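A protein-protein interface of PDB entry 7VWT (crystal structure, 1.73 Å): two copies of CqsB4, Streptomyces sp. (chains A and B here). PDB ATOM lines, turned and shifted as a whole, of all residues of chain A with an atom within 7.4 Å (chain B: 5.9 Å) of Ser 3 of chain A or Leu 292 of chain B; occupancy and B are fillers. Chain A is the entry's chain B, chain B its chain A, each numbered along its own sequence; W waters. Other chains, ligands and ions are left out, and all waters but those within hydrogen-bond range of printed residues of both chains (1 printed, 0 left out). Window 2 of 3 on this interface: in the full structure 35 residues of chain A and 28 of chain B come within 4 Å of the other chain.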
ATOM      1  N   PRO A   2       3.104   2.263   9.900  1.00  0.00           N
ATOM      2  CA  PRO A   2       3.800   3.548   9.702  1.00  0.00           C
ATOM      3  C   PRO A   2       3.354   4.616  10.705  1.00  0.00           C
ATOM      4  O   PRO A   2       2.393   5.340  10.481  1.00  0.00           O
ATOM      5  CB  PRO A   2       3.427   3.943   8.267  1.00  0.00           C
ATOM      6  CG  PRO A   2       2.176   3.164   7.973  1.00  0.00           C
ATOM      7  CD  PRO A   2       2.345   1.862   8.705  1.00  0.00           C
ATOM      8  N   SER A   3       4.100   4.706  11.799  1.00  0.00           N
ATOM      9  CA  SER A   3       3.770   5.445  13.007  1.00  0.00           C
ATOM     10  C   SER A   3       3.998   6.953  12.848  1.00  0.00           C
ATOM     11  O   SER A   3       4.703   7.413  11.948  1.00  0.00           O
ATOM     12  CB  SER A   3       4.643   4.939  14.147  1.00  0.00           C
ATOM     13  OG  SER A   3       5.951   5.454  13.950  1.00  0.00           O
ATOM     14  N   THR A   4       3.424   7.720  13.782  1.00  0.00           N
ATOM     15  CA  THR A   4       3.676   9.159  13.835  1.00  0.00           C
ATOM     16  C   THR A   4       5.168   9.447  13.967  1.00  0.00           C
ATOM     17  O   THR A   4       5.680  10.433  13.415  1.00  0.00           O
ATOM     18  CB  THR A   4       2.910   9.783  15.007  1.00  0.00           C
ATOM     19  OG1 THR A   4       1.561   9.309  15.013  1.00  0.00           O
ATOM     20  CG2 THR A   4       2.914  11.294  14.918  1.00  0.00           C
ATOM     21  N   VAL A   5       5.878   8.603  14.715  1.00  0.00           N
ATOM     22  CA  VAL A   5       7.323   8.744  14.868  1.00  0.00           C
ATOM     23  C   VAL A   5       8.031   8.556  13.531  1.00  0.00           C
ATOM     24  O   VAL A   5       8.939   9.319  13.169  1.00  0.00           O
ATOM     25  CB  VAL A   5       7.806   7.738  15.937  1.00  0.00           C
ATOM     26  CG1 VAL A   5       9.286   7.523  15.840  1.00  0.00           C
ATOM     27  CG2 VAL A   5       7.401   8.227  17.330  1.00  0.00           C
ATOM     28  N   GLN A   6       7.620   7.551  12.764  1.00  0.00           N
ATOM     29  CA  GLN A   6       8.212   7.347  11.449  1.00  0.00           C
ATOM     30  C   GLN A   6       7.845   8.461  10.479  1.00  0.00           C
ATOM     31  O   GLN A   6       8.653   8.792   9.608  1.00  0.00           O
ATOM     32  CB  GLN A   6       7.809   5.981  10.879  1.00  0.00           C
ATOM     33  CG  GLN A   6       8.379   4.792  11.692  1.00  0.00           C
ATOM     34  CD  GLN A   6       7.925   3.427  11.168  1.00  0.00           C
ATOM     35  OE1 GLN A   6       6.755   3.229  10.827  1.00  0.00           O
ATOM     36  NE2 GLN A   6       8.856   2.481  11.107  1.00  0.00           N
ATOM     37  N   GLU A   7       6.646   9.055  10.608  1.00  0.00           N
ATOM     38  CA  GLU A   7       6.275  10.183   9.743  1.00  0.00           C
ATOM     39  C   GLU A   7       7.113  11.430  10.045  1.00  0.00           C
ATOM     40  O   GLU A   7       7.517  12.158   9.119  1.00  0.00           O
ATOM     41  CB  GLU A   7       4.773  10.491   9.880  1.00  0.00           C
ATOM     42  CG  GLU A   7       3.866   9.426   9.214  1.00  0.00           C
ATOM     43  CD  GLU A   7       2.473   9.256   9.849  1.00  0.00           C
ATOM     44  OE1 GLU A   7       2.079  10.061  10.710  1.00  0.00           O
ATOM     45  OE2 GLU A   7       1.772   8.291   9.483  1.00  0.00           O
ATOM     46  N   LEU A   8       7.339  11.722  11.333  1.00  0.00           N
ATOM     47  CA  LEU A   8       8.227  12.821  11.707  1.00  0.00           C
ATOM     48  C   LEU A   8       9.643  12.583  11.197  1.00  0.00           C
ATOM     49  O   LEU A   8      10.320  13.522  10.765  1.00  0.00           O
ATOM     50  CB  LEU A   8       8.223  12.998  13.225  1.00  0.00           C
ATOM     51  CG  LEU A   8       6.961  13.632  13.793  1.00  0.00           C
ATOM     52  CD1 LEU A   8       6.879  13.385  15.284  1.00  0.00           C
ATOM     53  CD2 LEU A   8       6.925  15.139  13.418  1.00  0.00           C
ATOM     54  N   ASP A   9      10.096  11.324  11.221  1.00  0.00           N
ATOM     55  CA  ASP A   9      11.400  10.970  10.661  1.00  0.00           C
ATOM     56  C   ASP A   9      11.473  11.316   9.175  1.00  0.00           C
ATOM     57  O   ASP A   9      12.438  11.934   8.716  1.00  0.00           O
ATOM     58  CB  ASP A   9      11.669   9.480  10.859  1.00  0.00           C
ATOM     59  CG  ASP A   9      12.035   9.140  12.277  1.00  0.00           C
ATOM     60  OD1 ASP A   9      12.399  10.064  13.047  1.00  0.00           O
ATOM     61  OD2 ASP A   9      11.981   7.942  12.624  1.00  0.00           O
ATOM     62  N   LEU A  10      10.461  10.900   8.409  1.00  0.00           N
ATOM     63  CA  LEU A  10      10.427  11.170   6.975  1.00  0.00           C
ATOM     64  C   LEU A  10      10.403  12.665   6.690  1.00  0.00           C
ATOM     65  O   LEU A  10      10.965  13.122   5.683  1.00  0.00           O
ATOM     66  CB  LEU A  10       9.202  10.503   6.350  1.00  0.00           C
ATOM     67  CG  LEU A  10       9.253   8.980   6.339  1.00  0.00           C
ATOM     68  CD1 LEU A  10       7.891   8.394   5.923  1.00  0.00           C
ATOM     69  CD2 LEU A  10      10.347   8.557   5.369  1.00  0.00           C
ATOM     70  N   SER A  26      -1.069  15.606  16.818  1.00  0.00           N
ATOM     71  CA  SER A  26      -1.641  14.442  16.144  1.00  0.00           C
ATOM     72  C   SER A  26      -2.559  13.639  17.068  1.00  0.00           C
ATOM     73  O   SER A  26      -3.595  13.128  16.627  1.00  0.00           O
ATOM     74  CB  SER A  26      -0.503  13.579  15.609  1.00  0.00           C
ATOM     75  OG  SER A  26      -0.991  12.527  14.815  1.00  0.00           O
ATOM     76  N   ARG A  30      -6.623  13.020  16.487  1.00  0.00           N
ATOM     77  CA  ARG A  30      -7.247  11.705  16.576  1.00  0.00           C
ATOM     78  C   ARG A  30      -8.374  11.711  17.597  1.00  0.00           C
ATOM     79  O   ARG A  30      -9.402  11.054  17.403  1.00  0.00           O
ATOM     80  CB  ARG A  30      -6.207  10.651  16.958  1.00  0.00           C
ATOM     81  CG  ARG A  30      -6.724   9.244  16.870  1.00  0.00           C
ATOM     82  CD  ARG A  30      -5.854   8.301  17.679  1.00  0.00           C
ATOM     83  NE  ARG A  30      -4.468   8.762  17.775  1.00  0.00           N
ATOM     84  CZ  ARG A  30      -3.477   8.322  17.006  1.00  0.00           C
ATOM     85  NH1 ARG A  30      -3.731   7.413  16.068  1.00  0.00           N
ATOM     86  NH2 ARG A  30      -2.238   8.792  17.174  1.00  0.00           N
ATOM     87  N   ARG A  40      -7.070  12.257   5.819  1.00  0.00           N
ATOM     88  CA  ARG A  40      -5.716  12.349   6.368  1.00  0.00           C
ATOM     89  C   ARG A  40      -4.943  11.087   6.070  1.00  0.00           C
ATOM     90  O   ARG A  40      -3.733  11.137   5.842  1.00  0.00           O
ATOM     91  CB  ARG A  40      -5.737  12.605   7.892  1.00  0.00           C
ATOM     92  CG  ARG A  40      -6.304  11.457   8.732  1.00  0.00           C
ATOM     93  CD  ARG A  40      -5.828  11.512  10.179  1.00  0.00           C
ATOM     94  NE  ARG A  40      -4.364  11.591  10.326  1.00  0.00           N
ATOM     95  CZ  ARG A  40      -3.544  10.539  10.341  1.00  0.00           C
ATOM     96  NH1 ARG A  40      -4.040   9.305  10.197  1.00  0.00           N
ATOM     97  NH2 ARG A  40      -2.233  10.716  10.498  1.00  0.00           N
ATOM     98  N   TYR A  41      -5.641   9.946   6.018  1.00  0.00           N
ATOM     99  CA  TYR A  41      -4.997   8.674   5.743  1.00  0.00           C
ATOM    100  C   TYR A  41      -4.572   8.516   4.293  1.00  0.00           C
ATOM    101  O   TYR A  41      -3.884   7.539   3.984  1.00  0.00           O
ATOM    102  CB  TYR A  41      -5.934   7.529   6.135  1.00  0.00           C
ATOM    103  CG  TYR A  41      -6.151   7.411   7.618  1.00  0.00           C
ATOM    104  CD1 TYR A  41      -5.187   6.814   8.439  1.00  0.00           C
ATOM    105  CD2 TYR A  41      -7.314   7.897   8.203  1.00  0.00           C
ATOM    106  CE1 TYR A  41      -5.384   6.704   9.822  1.00  0.00           C
ATOM    107  CE2 TYR A  41      -7.523   7.803   9.580  1.00  0.00           C
ATOM    108  CZ  TYR A  41      -6.559   7.204  10.387  1.00  0.00           C
ATOM    109  OH  TYR A  41      -6.781   7.106  11.752  1.00  0.00           O
ATOM    110  N   PRO A  45       2.912  10.077   3.722  1.00  0.00           N
ATOM    111  CA  PRO A  45       3.296  10.006   5.145  1.00  0.00           C
ATOM    112  C   PRO A  45       4.282  11.087   5.589  1.00  0.00           C
ATOM    113  O   PRO A  45       4.224  11.515   6.751  1.00  0.00           O
ATOM    114  CB  PRO A  45       3.901   8.599   5.269  1.00  0.00           C
ATOM    115  CG  PRO A  45       3.230   7.798   4.168  1.00  0.00           C
ATOM    116  CD  PRO A  45       3.040   8.782   3.025  1.00  0.00           C
ATOM    117  N   ARG A  48       2.169  14.118   6.666  1.00  0.00           N
ATOM    118  CA  ARG A  48       1.096  14.005   7.638  1.00  0.00           C
ATOM    119  C   ARG A  48       1.320  14.856   8.883  1.00  0.00           C
ATOM    120  O   ARG A  48       0.316  15.317   9.451  1.00  0.00           O
ATOM    121  CB  ARG A  48       0.892  12.533   8.013  1.00  0.00           C
ATOM    122  CG  ARG A  48       0.224  11.724   6.905  1.00  0.00           C
ATOM    123  CD  ARG A  48      -0.192  10.309   7.350  1.00  0.00           C
ATOM    124  NE  ARG A  48      -0.306   9.445   6.177  1.00  0.00           N
ATOM    125  CZ  ARG A  48      -0.702   8.180   6.205  1.00  0.00           C
ATOM    126  NH1 ARG A  48      -1.014   7.599   7.358  1.00  0.00           N
ATOM    127  NH2 ARG A  48      -0.776   7.486   5.071  1.00  0.00           N
ATOM    128  N   GLU B 279      -4.944  -6.067  17.564  1.00  0.00           N
ATOM    129  CA  GLU B 279      -4.317  -4.789  17.226  1.00  0.00           C
ATOM    130  C   GLU B 279      -3.371  -4.306  18.317  1.00  0.00           C
ATOM    131  O   GLU B 279      -2.320  -3.731  18.002  1.00  0.00           O
ATOM    132  CB  GLU B 279      -5.377  -3.749  16.911  1.00  0.00           C
ATOM    133  CG  GLU B 279      -5.662  -3.747  15.406  1.00  0.00           C
ATOM    134  CD  GLU B 279      -6.992  -3.116  15.020  1.00  0.00           C
ATOM    135  OE1 GLU B 279      -7.657  -2.512  15.881  1.00  0.00           O
ATOM    136  OE2 GLU B 279      -7.367  -3.217  13.834  1.00  0.00           O
ATOM    137  N   ALA B 286       3.589  -3.415  19.572  1.00  0.00           N
ATOM    138  CA  ALA B 286       3.932  -2.144  18.930  1.00  0.00           C
ATOM    139  C   ALA B 286       2.967  -1.020  19.308  1.00  0.00           C
ATOM    140  O   ALA B 286       3.378   0.147  19.402  1.00  0.00           O
ATOM    141  CB  ALA B 286       3.963  -2.319  17.414  1.00  0.00           C
ATOM    142  N   PHE B 287       1.678  -1.350  19.497  1.00  0.00           N
ATOM    143  CA  PHE B 287       0.642  -0.393  19.904  1.00  0.00           C
ATOM    144  C   PHE B 287       1.080   0.468  21.091  1.00  0.00           C
ATOM    145  O   PHE B 287       0.830   1.685  21.125  1.00  0.00           O
ATOM    146  CB  PHE B 287      -0.637  -1.183  20.236  1.00  0.00           C
ATOM    147  CG  PHE B 287      -1.825  -0.346  20.654  1.00  0.00           C
ATOM    148  CD1 PHE B 287      -2.758   0.069  19.711  1.00  0.00           C
ATOM    149  CD2 PHE B 287      -2.031  -0.014  21.986  1.00  0.00           C
ATOM    150  CE1 PHE B 287      -3.867   0.840  20.089  1.00  0.00           C
ATOM    151  CE2 PHE B 287      -3.148   0.754  22.402  1.00  0.00           C
ATOM    152  CZ  PHE B 287      -4.080   1.180  21.430  1.00  0.00           C
ATOM    153  N   PHE B 288       1.745  -0.147  22.066  1.00  0.00           N
ATOM    154  CA  PHE B 288       2.156   0.528  23.289  1.00  0.00           C
ATOM    155  C   PHE B 288       3.534   1.202  23.186  1.00  0.00           C
ATOM    156  O   PHE B 288       3.877   2.028  24.050  1.00  0.00           O
ATOM    157  CB  PHE B 288       2.126  -0.498  24.444  1.00  0.00           C
ATOM    158  CG  PHE B 288       0.756  -1.128  24.655  1.00  0.00           C
ATOM    159  CD1 PHE B 288      -0.202  -0.478  25.393  1.00  0.00           C
ATOM    160  CD2 PHE B 288       0.432  -2.362  24.083  1.00  0.00           C
ATOM    161  CE1 PHE B 288      -1.474  -1.015  25.558  1.00  0.00           C
ATOM    162  CE2 PHE B 288      -0.845  -2.906  24.263  1.00  0.00           C
ATOM    163  CZ  PHE B 288      -1.787  -2.236  24.996  1.00  0.00           C
ATOM    164  N   SER B 290       4.849   2.980  20.402  1.00  0.00           N
ATOM    165  CA  SER B 290       4.872   4.164  19.558  1.00  0.00           C
ATOM    166  C   SER B 290       3.442   4.620  19.348  1.00  0.00           C
ATOM    167  O   SER B 290       2.516   3.809  19.421  1.00  0.00           O
ATOM    168  CB  SER B 290       5.505   3.878  18.187  1.00  0.00           C
ATOM    169  OG  SER B 290       6.667   3.083  18.305  1.00  0.00           O
ATOM    170  N   PRO B 291       3.229   5.913  19.063  1.00  0.00           N
ATOM    171  CA  PRO B 291       1.890   6.352  18.633  1.00  0.00           C
ATOM    172  C   PRO B 291       1.595   5.841  17.232  1.00  0.00           C
ATOM    173  O   PRO B 291       2.064   6.421  16.242  1.00  0.00           O
ATOM    174  CB  PRO B 291       1.982   7.881  18.683  1.00  0.00           C
ATOM    175  CG  PRO B 291       3.433   8.153  18.471  1.00  0.00           C
ATOM    176  CD  PRO B 291       4.206   7.013  19.070  1.00  0.00           C
ATOM    177  N   LEU B 292       0.861   4.738  17.119  1.00  0.00           N
ATOM    178  CA  LEU B 292       0.644   4.141  15.803  1.00  0.00           C
ATOM    179  C   LEU B 292      -0.435   4.881  15.009  1.00  0.00           C
ATOM    180  O   LEU B 292      -1.382   5.448  15.565  1.00  0.00           O
ATOM    181  CB  LEU B 292       0.259   2.664  15.933  1.00  0.00           C
ATOM    182  CG  LEU B 292       1.375   1.776  16.488  1.00  0.00           C
ATOM    183  CD1 LEU B 292       1.023   0.289  16.413  1.00  0.00           C
ATOM    184  CD2 LEU B 292       2.698   2.077  15.759  1.00  0.00           C
ATOM    185  N   ASP B 293      -0.295   4.840  13.685  1.00  0.00           N
ATOM    186  CA  ASP B 293      -1.185   5.534  12.755  1.00  0.00           C
ATOM    187  C   ASP B 293      -1.877   4.469  11.899  1.00  0.00           C
ATOM    188  O   ASP B 293      -1.275   3.935  10.962  1.00  0.00           O
ATOM    189  CB  ASP B 293      -0.402   6.523  11.888  1.00  0.00           C
ATOM    190  CG  ASP B 293      -1.297   7.301  10.907  1.00  0.00           C
ATOM    191  OD1 ASP B 293      -0.790   8.259  10.286  1.00  0.00           O
ATOM    192  OD2 ASP B 293      -2.501   6.967  10.762  1.00  0.00           O
ATOM    193  N   PHE B 294      -3.134   4.164  12.212  1.00  0.00           N
ATOM    194  CA  PHE B 294      -3.819   3.081  11.515  1.00  0.00           C
ATOM    195  C   PHE B 294      -5.323   3.254  11.674  1.00  0.00           C
ATOM    196  O   PHE B 294      -5.796   3.940  12.591  1.00  0.00           O
ATOM    197  CB  PHE B 294      -3.369   1.701  12.042  1.00  0.00           C
ATOM    198  CG  PHE B 294      -3.753   1.433  13.496  1.00  0.00           C
ATOM    199  CD1 PHE B 294      -4.907   0.710  13.808  1.00  0.00           C
ATOM    200  CD2 PHE B 294      -2.959   1.898  14.542  1.00  0.00           C
ATOM    201  CE1 PHE B 294      -5.265   0.466  15.142  1.00  0.00           C
ATOM    202  CE2 PHE B 294      -3.306   1.656  15.871  1.00  0.00           C
ATOM    203  CZ  PHE B 294      -4.463   0.940  16.171  1.00  0.00           C
HETATM  204  O   HOH W   1       0.377  10.085  12.897  1.00  0.00           O
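No position is printed for both chains. Of the 11 pairs that touch across the chains among the printed residues, none has its exchanged pair printed and touching as well.
Pro 2 of chain A touches Asp 293 of chain B (O to CB, 3.3 Å). Pro 291 of chain B touches Ser 3 of chain A (O to CB, 3.6 Å). CB of Ser 3 of chain A touches CD2 of Leu 292 of chain B, 3.8 Å away. Pro 291 of chain B touches Val 5 of chain A. CE1 of Tyr 41 of chain A touches OD2 of Asp 293 of chain B, at 3.0 Å.
Water W1 lies within hydrogen-bond range of the side-chain hydroxyl of Thr 4 of chain A (2.5 Å), the side-chain carboxylate of Glu 7 of chain A (2.8 Å), the side-chain carboxylate of Asp 293 of chain B (3.4 Å) and the side-chain hydroxyl of Ser 26 of chain A (3.4 Å).
Hydrophobic or aromatic side chains of chain A within 4 Å of the printed part of chain B: Val 5 and Tyr 41. Of the 9 printed residues of chain B, 4 touch a printed residue of chain A. Printed residues of chain B that touch a printed residue of chain A: Pro 291, Leu 292, Asp 293 and Phe 294. Hydrophobic or aromatic side chains of chain B that line the printed part of chain A: Pro 291 and Leu 292. Among the printed residues, Asp or Glu carboxylates within 4 Å of a Lys or Arg side-chain nitrogen of the other chain: Arg 40 of chain A with Asp 293 of chain B (2.9 Å) and Arg 48 of chain A with Asp 293 of chain B (3.0 Å).
NH1 of Arg 48 of chain A is in salt-bridge range of OE2 of Glu 7 of chain A (3.6 Å). The guanidinium group (NH2) of Arg 48 of chain A sits at hydrogen-bond distance from the backbone carbonyl oxygen (O) of Tyr 41 of chain A (3.3 Å). OG of Ser 3 of chain A is in hydrogen-bond range of N of Gln 6 of chain A, 2.9 Å away. N of Val 5 of chain A sits close to OG of Ser 3 of chain A (3.2 Å).
O of Leu 292 of chain B sits at hydrogen-bond distance from NH1 of Arg 30 of chain A, 3.1 Å away. OD2 of Asp 293 of chain B lies within salt-bridge range of NH1 of Arg 40 of chain A, at 2.9 Å. The backbone NH of Thr 4 of chain A is in hydrogen-bond range of the backbone carbonyl oxygen of Pro 291 of chain B (3.1 Å). The side-chain carboxylate (OD1) of Asp 293 of chain B sits close to the side-chain carboxylate (OE2) of Glu 7 of chain A (2.7 Å). OD1 of Asp 293 of chain B lies within salt-bridge range of NH1 of Arg 48 of chain A (3.0 Å). The backbone carbonyl oxygen of Phe 294 of chain B is in hydrogen-bond range of the side-chain hydroxyl of Tyr 41 of chain A (3.4 Å).
Of the printed residues of chain B, Pro 2 of chain A touches Asp 293 (3.3 Å). Of chain B, only Pro 291 (3.6 Å) and Leu 292 (3.8 Å) come within 4 Å of Ser 3 of chain A. Printed residues of chain B within 4 Å of Thr 4 of chain A: Pro 291 (3.1 Å). Of the printed residues of chain B, Val 5 of chain A touches Pro 291 (3.8 Å). Of the printed residues of chain B, Arg 48 of chain A touches Asp 293 (3.0 Å). Of chain A, only Ser 3 and Arg 30 come within 4 Å of Leu 292 of chain B. The nearest residue of chain B that does not touch Ser 3 of chain A is Asp 293 of chain B (4.2 Å). The nearest residue of chain A that does not touch Leu 292 of chain B is Thr 4 of chain A (4.9 Å).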
